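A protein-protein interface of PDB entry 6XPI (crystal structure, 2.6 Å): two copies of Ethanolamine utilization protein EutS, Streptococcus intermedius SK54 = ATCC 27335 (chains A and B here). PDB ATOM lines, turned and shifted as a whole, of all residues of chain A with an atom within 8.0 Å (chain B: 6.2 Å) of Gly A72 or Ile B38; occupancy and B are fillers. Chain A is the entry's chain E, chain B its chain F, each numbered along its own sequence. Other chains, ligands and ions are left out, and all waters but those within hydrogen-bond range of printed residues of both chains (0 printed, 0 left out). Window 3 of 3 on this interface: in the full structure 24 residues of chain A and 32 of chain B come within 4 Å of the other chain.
No position is printed for both chains. Of the 8 pairs that touch across the chains among the printed residues, none has its exchanged pair printed and touching as well.
Of the printed residues of chain B, Ile A65 touches Val B41. Printed residues of chain B within 4 Å of Ala A68: Ile B38. Of chain B, only Ile B38 comes within 4 Å of Gly A72. Ser A101 touches none of the printed residues of chain B. Of the printed residues of chain A, Ile B34 touches Asp A69 (3.5 Å). Printed residues of chain A within 4 Å of Ala B36: Asp A69 (3.9 Å). Ile B38 touches just these residues of chain A: Ala A68, Asp A69 and Gly A72. Printed residues of chain A within 4 Å of Val B41: Ile A65 (3.6 Å) and Asp A69 (3.7 Å). Glu B43 touches none of the printed residues of chain A.
Hydrophobic or aromatic side chains of chain A that line the printed part of chain B: Ile A65. Of the 9 printed residues of chain B, 5 touch a printed residue of chain A. Hydrophobic or aromatic side chains of chain B within 4 Å of the printed part of chain A: Ile B34, Ile B38 and Val B41.
Among the printed residues, merely in contact across the chains: Asp A69 with Ile B34, Gly A72 with Ile B38, Ala A68 with Ile B38, Ile A65 with Val B41, Asp A69 with Ile B38, Asp A69 with Val B41, Asp A69 with Pro B37 and Asp A69 with Ala B36.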
ATOM      1  N   ILE A  65      -1.720  -8.402  13.027  1.00  0.00           N
ATOM      2  CA  ILE A  65      -0.698  -7.751  13.816  1.00  0.00           C
ATOM      3  C   ILE A  65       0.685  -8.264  13.455  1.00  0.00           C
ATOM      4  O   ILE A  65       1.612  -7.472  13.363  1.00  0.00           O
ATOM      5  CB  ILE A  65      -0.994  -7.808  15.337  1.00  0.00           C
ATOM      6  CG1 ILE A  65      -0.108  -6.805  16.105  1.00  0.00           C
ATOM      7  CG2 ILE A  65      -0.843  -9.208  15.898  1.00  0.00           C
ATOM      8  CD1 ILE A  65      -0.134  -5.359  15.488  1.00  0.00           C
ATOM      9  N   ILE A  66       0.810  -9.570  13.174  1.00  0.00           N
ATOM     10  CA  ILE A  66       2.070 -10.193  12.794  1.00  0.00           C
ATOM     11  C   ILE A  66       2.512  -9.664  11.446  1.00  0.00           C
ATOM     12  O   ILE A  66       3.668  -9.282  11.304  1.00  0.00           O
ATOM     13  CB  ILE A  66       1.932 -11.729  12.781  1.00  0.00           C
ATOM     14  CG1 ILE A  66       1.424 -12.257  14.132  1.00  0.00           C
ATOM     15  CG2 ILE A  66       3.237 -12.382  12.374  1.00  0.00           C
ATOM     16  CD1 ILE A  66       1.035 -13.701  14.109  1.00  0.00           C
ATOM     17  N   ALA A  67       1.591  -9.608  10.469  1.00  0.00           N
ATOM     18  CA  ALA A  67       1.873  -9.123   9.128  1.00  0.00           C
ATOM     19  C   ALA A  67       2.223  -7.648   9.121  1.00  0.00           C
ATOM     20  O   ALA A  67       3.083  -7.256   8.343  1.00  0.00           O
ATOM     21  CB  ALA A  67       0.700  -9.399   8.207  1.00  0.00           C
ATOM     22  N   ALA A  68       1.625  -6.837  10.009  1.00  0.00           N
ATOM     23  CA  ALA A  68       1.967  -5.414  10.083  1.00  0.00           C
ATOM     24  C   ALA A  68       3.423  -5.266  10.544  1.00  0.00           C
ATOM     25  O   ALA A  68       4.172  -4.503   9.948  1.00  0.00           O
ATOM     26  CB  ALA A  68       1.039  -4.681  11.041  1.00  0.00           C
ATOM     27  N   ASP A  69       3.826  -6.042  11.570  1.00  0.00           N
ATOM     28  CA  ASP A  69       5.163  -6.079  12.139  1.00  0.00           C
ATOM     29  C   ASP A  69       6.189  -6.361  11.045  1.00  0.00           C
ATOM     30  O   ASP A  69       7.040  -5.518  10.803  1.00  0.00           O
ATOM     31  CB  ASP A  69       5.226  -7.112  13.301  1.00  0.00           C
ATOM     32  CG  ASP A  69       6.621  -7.553  13.740  1.00  0.00           C
ATOM     33  OD1 ASP A  69       7.399  -6.692  14.237  1.00  0.00           O
ATOM     34  OD2 ASP A  69       6.928  -8.762  13.614  1.00  0.00           O
ATOM     35  N   ILE A  70       6.041  -7.481  10.326  1.00  0.00           N
ATOM     36  CA  ILE A  70       6.934  -7.893   9.253  1.00  0.00           C
ATOM     37  C   ILE A  70       6.982  -6.893   8.092  1.00  0.00           C
ATOM     38  O   ILE A  70       8.060  -6.655   7.545  1.00  0.00           O
ATOM     39  CB  ILE A  70       6.537  -9.308   8.817  1.00  0.00           C
ATOM     40  CG1 ILE A  70       6.778 -10.281   9.962  1.00  0.00           C
ATOM     41  CG2 ILE A  70       7.268  -9.749   7.558  1.00  0.00           C
ATOM     42  CD1 ILE A  70       5.910 -11.387   9.931  1.00  0.00           C
ATOM     43  N   ALA A  71       5.832  -6.265   7.744  1.00  0.00           N
ATOM     44  CA  ALA A  71       5.790  -5.247   6.683  1.00  0.00           C
ATOM     45  C   ALA A  71       6.595  -4.007   7.139  1.00  0.00           C
ATOM     46  O   ALA A  71       7.440  -3.512   6.389  1.00  0.00           O
ATOM     47  CB  ALA A  71       4.353  -4.872   6.352  1.00  0.00           C
ATOM     48  N   GLY A  72       6.393  -3.594   8.396  1.00  0.00           N
ATOM     49  CA  GLY A  72       7.121  -2.491   9.020  1.00  0.00           C
ATOM     50  C   GLY A  72       8.605  -2.778   9.221  1.00  0.00           C
ATOM     51  O   GLY A  72       9.418  -1.859   9.352  1.00  0.00           O
ATOM     52  N   ALA A  73       8.976  -4.063   9.241  1.00  0.00           N
ATOM     53  CA  ALA A  73      10.364  -4.467   9.298  1.00  0.00           C
ATOM     54  C   ALA A  73      11.051  -4.270   7.919  1.00  0.00           C
ATOM     55  O   ALA A  73      12.155  -4.755   7.746  1.00  0.00           O
ATOM     56  CB  ALA A  73      10.462  -5.916   9.731  1.00  0.00           C
ATOM     57  N   ALA A  74      10.399  -3.560   6.948  1.00  0.00           N
ATOM     58  CA  ALA A  74      10.920  -3.207   5.622  1.00  0.00           C
ATOM     59  C   ALA A  74      10.545  -1.761   5.176  1.00  0.00           C
ATOM     60  O   ALA A  74       9.563  -1.169   5.613  1.00  0.00           O
ATOM     61  CB  ALA A  74      10.535  -4.235   4.580  1.00  0.00           C
ATOM     62  N   ALA A  75      11.411  -1.202   4.345  1.00  0.00           N
ATOM     63  CA  ALA A  75      11.519   0.178   3.862  1.00  0.00           C
ATOM     64  C   ALA A  75      10.305   1.102   4.067  1.00  0.00           C
ATOM     65  O   ALA A  75       9.175   0.676   3.837  1.00  0.00           O
ATOM     66  CB  ALA A  75      11.928   0.194   2.388  1.00  0.00           C
ATOM     67  N   ASN A  76      10.593   2.381   4.487  1.00  0.00           N
ATOM     68  CA  ASN A  76       9.770   3.609   4.578  1.00  0.00           C
ATOM     69  C   ASN A  76       8.217   3.410   4.640  1.00  0.00           C
ATOM     70  O   ASN A  76       7.486   4.214   4.061  1.00  0.00           O
ATOM     71  CB  ASN A  76      10.099   4.442   3.289  1.00  0.00           C
ATOM     72  CG  ASN A  76      10.598   5.872   3.433  1.00  0.00           C
ATOM     73  OD1 ASN A  76       9.812   6.833   3.448  1.00  0.00           O
ATOM     74  ND2 ASN A  76      11.917   6.057   3.445  1.00  0.00           N
ATOM     75  N   ILE A  77       7.719   2.389   5.345  1.00  0.00           N
ATOM     76  CA  ILE A  77       6.295   2.079   5.351  1.00  0.00           C
ATOM     77  C   ILE A  77       5.498   2.918   6.349  1.00  0.00           C
ATOM     78  O   ILE A  77       5.971   3.210   7.448  1.00  0.00           O
ATOM     79  CB  ILE A  77       6.085   0.545   5.539  1.00  0.00           C
ATOM     80  CG1 ILE A  77       6.305  -0.199   4.220  1.00  0.00           C
ATOM     81  CG2 ILE A  77       4.726   0.172   6.121  1.00  0.00           C
ATOM     82  CD1 ILE A  77       5.498   0.300   3.047  1.00  0.00           C
ATOM     83  N   ASP A  78       4.276   3.310   5.935  1.00  0.00           N
ATOM     84  CA  ASP A  78       3.320   4.051   6.749  1.00  0.00           C
ATOM     85  C   ASP A  78       2.094   3.160   6.905  1.00  0.00           C
ATOM     86  O   ASP A  78       1.374   2.956   5.933  1.00  0.00           O
ATOM     87  CB  ASP A  78       2.946   5.375   6.071  1.00  0.00           C
ATOM     88  CG  ASP A  78       4.149   6.276   5.859  1.00  0.00           C
ATOM     89  OD1 ASP A  78       4.926   6.473   6.831  1.00  0.00           O
ATOM     90  OD2 ASP A  78       4.330   6.774   4.715  1.00  0.00           O
ATOM     91  N   ILE A  79       1.897   2.569   8.093  1.00  0.00           N
ATOM     92  CA  ILE A  79       0.763   1.685   8.332  1.00  0.00           C
ATOM     93  C   ILE A  79      -0.491   2.519   8.333  1.00  0.00           C
ATOM     94  O   ILE A  79      -0.630   3.422   9.160  1.00  0.00           O
ATOM     95  CB  ILE A  79       0.878   0.886   9.661  1.00  0.00           C
ATOM     96  CG1 ILE A  79       2.138  -0.006   9.723  1.00  0.00           C
ATOM     97  CG2 ILE A  79      -0.368   0.082   9.918  1.00  0.00           C
ATOM     98  CD1 ILE A  79       2.201  -1.129   8.721  1.00  0.00           C
ATOM     99  N   VAL A  82      -4.195  -1.618  10.840  1.00  0.00           N
ATOM    100  CA  VAL A  82      -3.944  -2.993  11.253  1.00  0.00           C
ATOM    101  C   VAL A  82      -5.281  -3.377  11.811  1.00  0.00           C
ATOM    102  O   VAL A  82      -5.622  -2.928  12.896  1.00  0.00           O
ATOM    103  CB  VAL A  82      -2.868  -3.125  12.359  1.00  0.00           C
ATOM    104  CG1 VAL A  82      -2.452  -4.573  12.529  1.00  0.00           C
ATOM    105  CG2 VAL A  82      -1.660  -2.259  12.082  1.00  0.00           C
ATOM    106  N   VAL A  89      -4.601  -5.603   6.493  1.00  0.00           N
ATOM    107  CA  VAL A  89      -3.497  -4.676   6.719  1.00  0.00           C
ATOM    108  C   VAL A  89      -3.354  -3.780   5.487  1.00  0.00           C
ATOM    109  O   VAL A  89      -3.334  -4.282   4.360  1.00  0.00           O
ATOM    110  CB  VAL A  89      -2.138  -5.376   7.005  1.00  0.00           C
ATOM    111  CG1 VAL A  89      -1.072  -4.352   7.396  1.00  0.00           C
ATOM    112  CG2 VAL A  89      -2.277  -6.452   8.070  1.00  0.00           C
ATOM    113  N   PHE A  91      -0.934  -0.352   3.819  1.00  0.00           N
ATOM    114  CA  PHE A  91       0.249   0.485   4.003  1.00  0.00           C
ATOM    115  C   PHE A  91       0.617   1.331   2.760  1.00  0.00           C
ATOM    116  O   PHE A  91       0.347   0.946   1.628  1.00  0.00           O
ATOM    117  CB  PHE A  91       1.443  -0.317   4.516  1.00  0.00           C
ATOM    118  CG  PHE A  91       1.710  -1.634   3.839  1.00  0.00           C
ATOM    119  CD1 PHE A  91       2.504  -1.702   2.708  1.00  0.00           C
ATOM    120  CD2 PHE A  91       1.248  -2.813   4.381  1.00  0.00           C
ATOM    121  CE1 PHE A  91       2.798  -2.925   2.113  1.00  0.00           C
ATOM    122  CE2 PHE A  91       1.538  -4.032   3.782  1.00  0.00           C
ATOM    123  CZ  PHE A  91       2.320  -4.084   2.661  1.00  0.00           C
ATOM    124  N   SER A 101       7.625  -5.283   1.295  1.00  0.00           N
ATOM    125  CA  SER A 101       6.820  -5.617   2.469  1.00  0.00           C
ATOM    126  C   SER A 101       5.923  -6.805   2.184  1.00  0.00           C
ATOM    127  O   SER A 101       5.891  -7.743   2.971  1.00  0.00           O
ATOM    128  CB  SER A 101       5.979  -4.421   2.903  1.00  0.00           C
ATOM    129  OG  SER A 101       6.815  -3.337   3.259  1.00  0.00           O
ATOM    130  N   ASP A 104       7.904 -10.086   1.858  1.00  0.00           N
ATOM    131  CA  ASP A 104       8.349 -10.570   3.152  1.00  0.00           C
ATOM    132  C   ASP A 104       7.220 -11.194   3.947  1.00  0.00           C
ATOM    133  O   ASP A 104       7.453 -12.166   4.668  1.00  0.00           O
ATOM    134  CB  ASP A 104       9.036  -9.452   3.936  1.00  0.00           C
ATOM    135  CG  ASP A 104      10.443  -9.196   3.427  1.00  0.00           C
ATOM    136  OD1 ASP A 104      10.614  -9.079   2.183  1.00  0.00           O
ATOM    137  OD2 ASP A 104      11.380  -9.119   4.267  1.00  0.00           O
ATOM    138  N   ILE A 105       6.000 -10.655   3.811  1.00  0.00           N
ATOM    139  CA  ILE A 105       4.820 -11.185   4.482  1.00  0.00           C
ATOM    140  C   ILE A 105       4.530 -12.567   3.908  1.00  0.00           C
ATOM    141  O   ILE A 105       4.407 -13.524   4.661  1.00  0.00           O
ATOM    142  CB  ILE A 105       3.624 -10.220   4.313  1.00  0.00           C
ATOM    143  CG1 ILE A 105       3.831  -8.954   5.131  1.00  0.00           C
ATOM    144  CG2 ILE A 105       2.319 -10.894   4.695  1.00  0.00           C
ATOM    145  CD1 ILE A 105       2.875  -7.868   4.774  1.00  0.00           C
ATOM    146  N   ILE B  34       5.860 -12.003  19.239  1.00  0.00           N
ATOM    147  CA  ILE B  34       6.583 -11.068  18.399  1.00  0.00           C
ATOM    148  C   ILE B  34       7.629 -10.527  19.348  1.00  0.00           C
ATOM    149  O   ILE B  34       7.292  -9.745  20.239  1.00  0.00           O
ATOM    150  CB  ILE B  34       5.659  -9.966  17.851  1.00  0.00           C
ATOM    151  CG1 ILE B  34       4.516 -10.580  17.019  1.00  0.00           C
ATOM    152  CG2 ILE B  34       6.466  -8.949  17.049  1.00  0.00           C
ATOM    153  CD1 ILE B  34       3.493  -9.611  16.590  1.00  0.00           C
ATOM    154  N   ALA B  36      10.259  -8.500  19.169  1.00  0.00           N
ATOM    155  CA  ALA B  36      10.548  -7.071  19.208  1.00  0.00           C
ATOM    156  C   ALA B  36       9.650  -6.341  18.255  1.00  0.00           C
ATOM    157  O   ALA B  36      10.020  -6.075  17.114  1.00  0.00           O
ATOM    158  CB  ALA B  36      11.996  -6.805  18.850  1.00  0.00           C
ATOM    159  N   PRO B  37       8.421  -6.045  18.695  1.00  0.00           N
ATOM    160  CA  PRO B  37       7.484  -5.350  17.799  1.00  0.00           C
ATOM    161  C   PRO B  37       7.996  -3.985  17.357  1.00  0.00           C
ATOM    162  O   PRO B  37       8.800  -3.361  18.045  1.00  0.00           O
ATOM    163  CB  PRO B  37       6.222  -5.218  18.647  1.00  0.00           C
ATOM    164  CG  PRO B  37       6.360  -6.265  19.713  1.00  0.00           C
ATOM    165  CD  PRO B  37       7.811  -6.339  20.009  1.00  0.00           C
ATOM    166  N   ILE B  38       7.559  -3.545  16.183  1.00  0.00           N
ATOM    167  CA  ILE B  38       7.903  -2.228  15.659  1.00  0.00           C
ATOM    168  C   ILE B  38       7.033  -1.180  16.375  1.00  0.00           C
ATOM    169  O   ILE B  38       5.921  -1.493  16.806  1.00  0.00           O
ATOM    170  CB  ILE B  38       7.691  -2.203  14.126  1.00  0.00           C
ATOM    171  CG1 ILE B  38       6.252  -2.621  13.766  1.00  0.00           C
ATOM    172  CG2 ILE B  38       8.700  -3.115  13.447  1.00  0.00           C
ATOM    173  CD1 ILE B  38       5.857  -2.463  12.318  1.00  0.00           C
ATOM    174  N   GLU B  39       7.524   0.062  16.489  1.00  0.00           N
ATOM    175  CA  GLU B  39       6.795   1.135  17.174  1.00  0.00           C
ATOM    176  C   GLU B  39       5.351   1.346  16.651  1.00  0.00           C
ATOM    177  O   GLU B  39       4.476   1.730  17.428  1.00  0.00           O
ATOM    178  CB  GLU B  39       7.605   2.449  17.152  1.00  0.00           C
ATOM    179  CG  GLU B  39       9.051   2.312  17.634  1.00  0.00           C
ATOM    180  CD  GLU B  39       9.311   1.947  19.094  1.00  0.00           C
ATOM    181  OE1 GLU B  39       9.573   2.871  19.902  1.00  0.00           O
ATOM    182  OE2 GLU B  39       9.295   0.736  19.424  1.00  0.00           O
ATOM    183  N   ALA B  40       5.098   1.068  15.354  1.00  0.00           N
ATOM    184  CA  ALA B  40       3.767   1.198  14.762  1.00  0.00           C
ATOM    185  C   ALA B  40       2.812   0.145  15.323  1.00  0.00           C
ATOM    186  O   ALA B  40       1.641   0.425  15.526  1.00  0.00           O
ATOM    187  CB  ALA B  40       3.847   1.052  13.255  1.00  0.00           C
ATOM    188  N   VAL B  41       3.307  -1.060  15.558  1.00  0.00           N
ATOM    189  CA  VAL B  41       2.529  -2.150  16.121  1.00  0.00           C
ATOM    190  C   VAL B  41       2.180  -1.832  17.588  1.00  0.00           C
ATOM    191  O   VAL B  41       1.050  -2.064  18.017  1.00  0.00           O
ATOM    192  CB  VAL B  41       3.333  -3.460  15.931  1.00  0.00           C
ATOM    193  CG1 VAL B  41       3.063  -4.492  17.032  1.00  0.00           C
ATOM    194  CG2 VAL B  41       3.077  -4.037  14.542  1.00  0.00           C
ATOM    195  N   TYR B  42       3.136  -1.261  18.341  1.00  0.00           N
ATOM    196  CA  TYR B  42       2.904  -0.836  19.717  1.00  0.00           C
ATOM    197  C   TYR B  42       1.834   0.279  19.716  1.00  0.00           C
ATOM    198  O   TYR B  42       0.928   0.270  20.546  1.00  0.00           O
ATOM    199  CB  TYR B  42       4.197  -0.273  20.341  1.00  0.00           C
ATOM    200  CG  TYR B  42       5.276  -1.275  20.689  1.00  0.00           C
ATOM    201  CD1 TYR B  42       4.997  -2.380  21.476  1.00  0.00           C
ATOM    202  CD2 TYR B  42       6.599  -1.047  20.339  1.00  0.00           C
ATOM    203  CE1 TYR B  42       5.994  -3.273  21.846  1.00  0.00           C
ATOM    204  CE2 TYR B  42       7.607  -1.926  20.712  1.00  0.00           C
ATOM    205  CZ  TYR B  42       7.298  -3.046  21.457  1.00  0.00           C
ATOM    206  OH  TYR B  42       8.282  -3.931  21.831  1.00  0.00           O
ATOM    207  N   GLU B  43       1.938   1.221  18.761  1.00  0.00           N
ATOM    208  CA  GLU B  43       1.014   2.336  18.624  1.00  0.00           C
ATOM    209  C   GLU B  43      -0.406   1.907  18.196  1.00  0.00           C
ATOM    210  O   GLU B  43      -1.364   2.236  18.894  1.00  0.00           O
ATOM    211  CB  GLU B  43       1.589   3.412  17.694  1.00  0.00           C
ATOM    212  CG  GLU B  43       1.095   4.810  18.018  1.00  0.00           C
ATOM    213  CD  GLU B  43       1.615   5.382  19.324  1.00  0.00           C
ATOM    214  OE1 GLU B  43       2.566   6.197  19.274  1.00  0.00           O
ATOM    215  OE2 GLU B  43       1.068   5.031  20.396  1.00  0.00           O
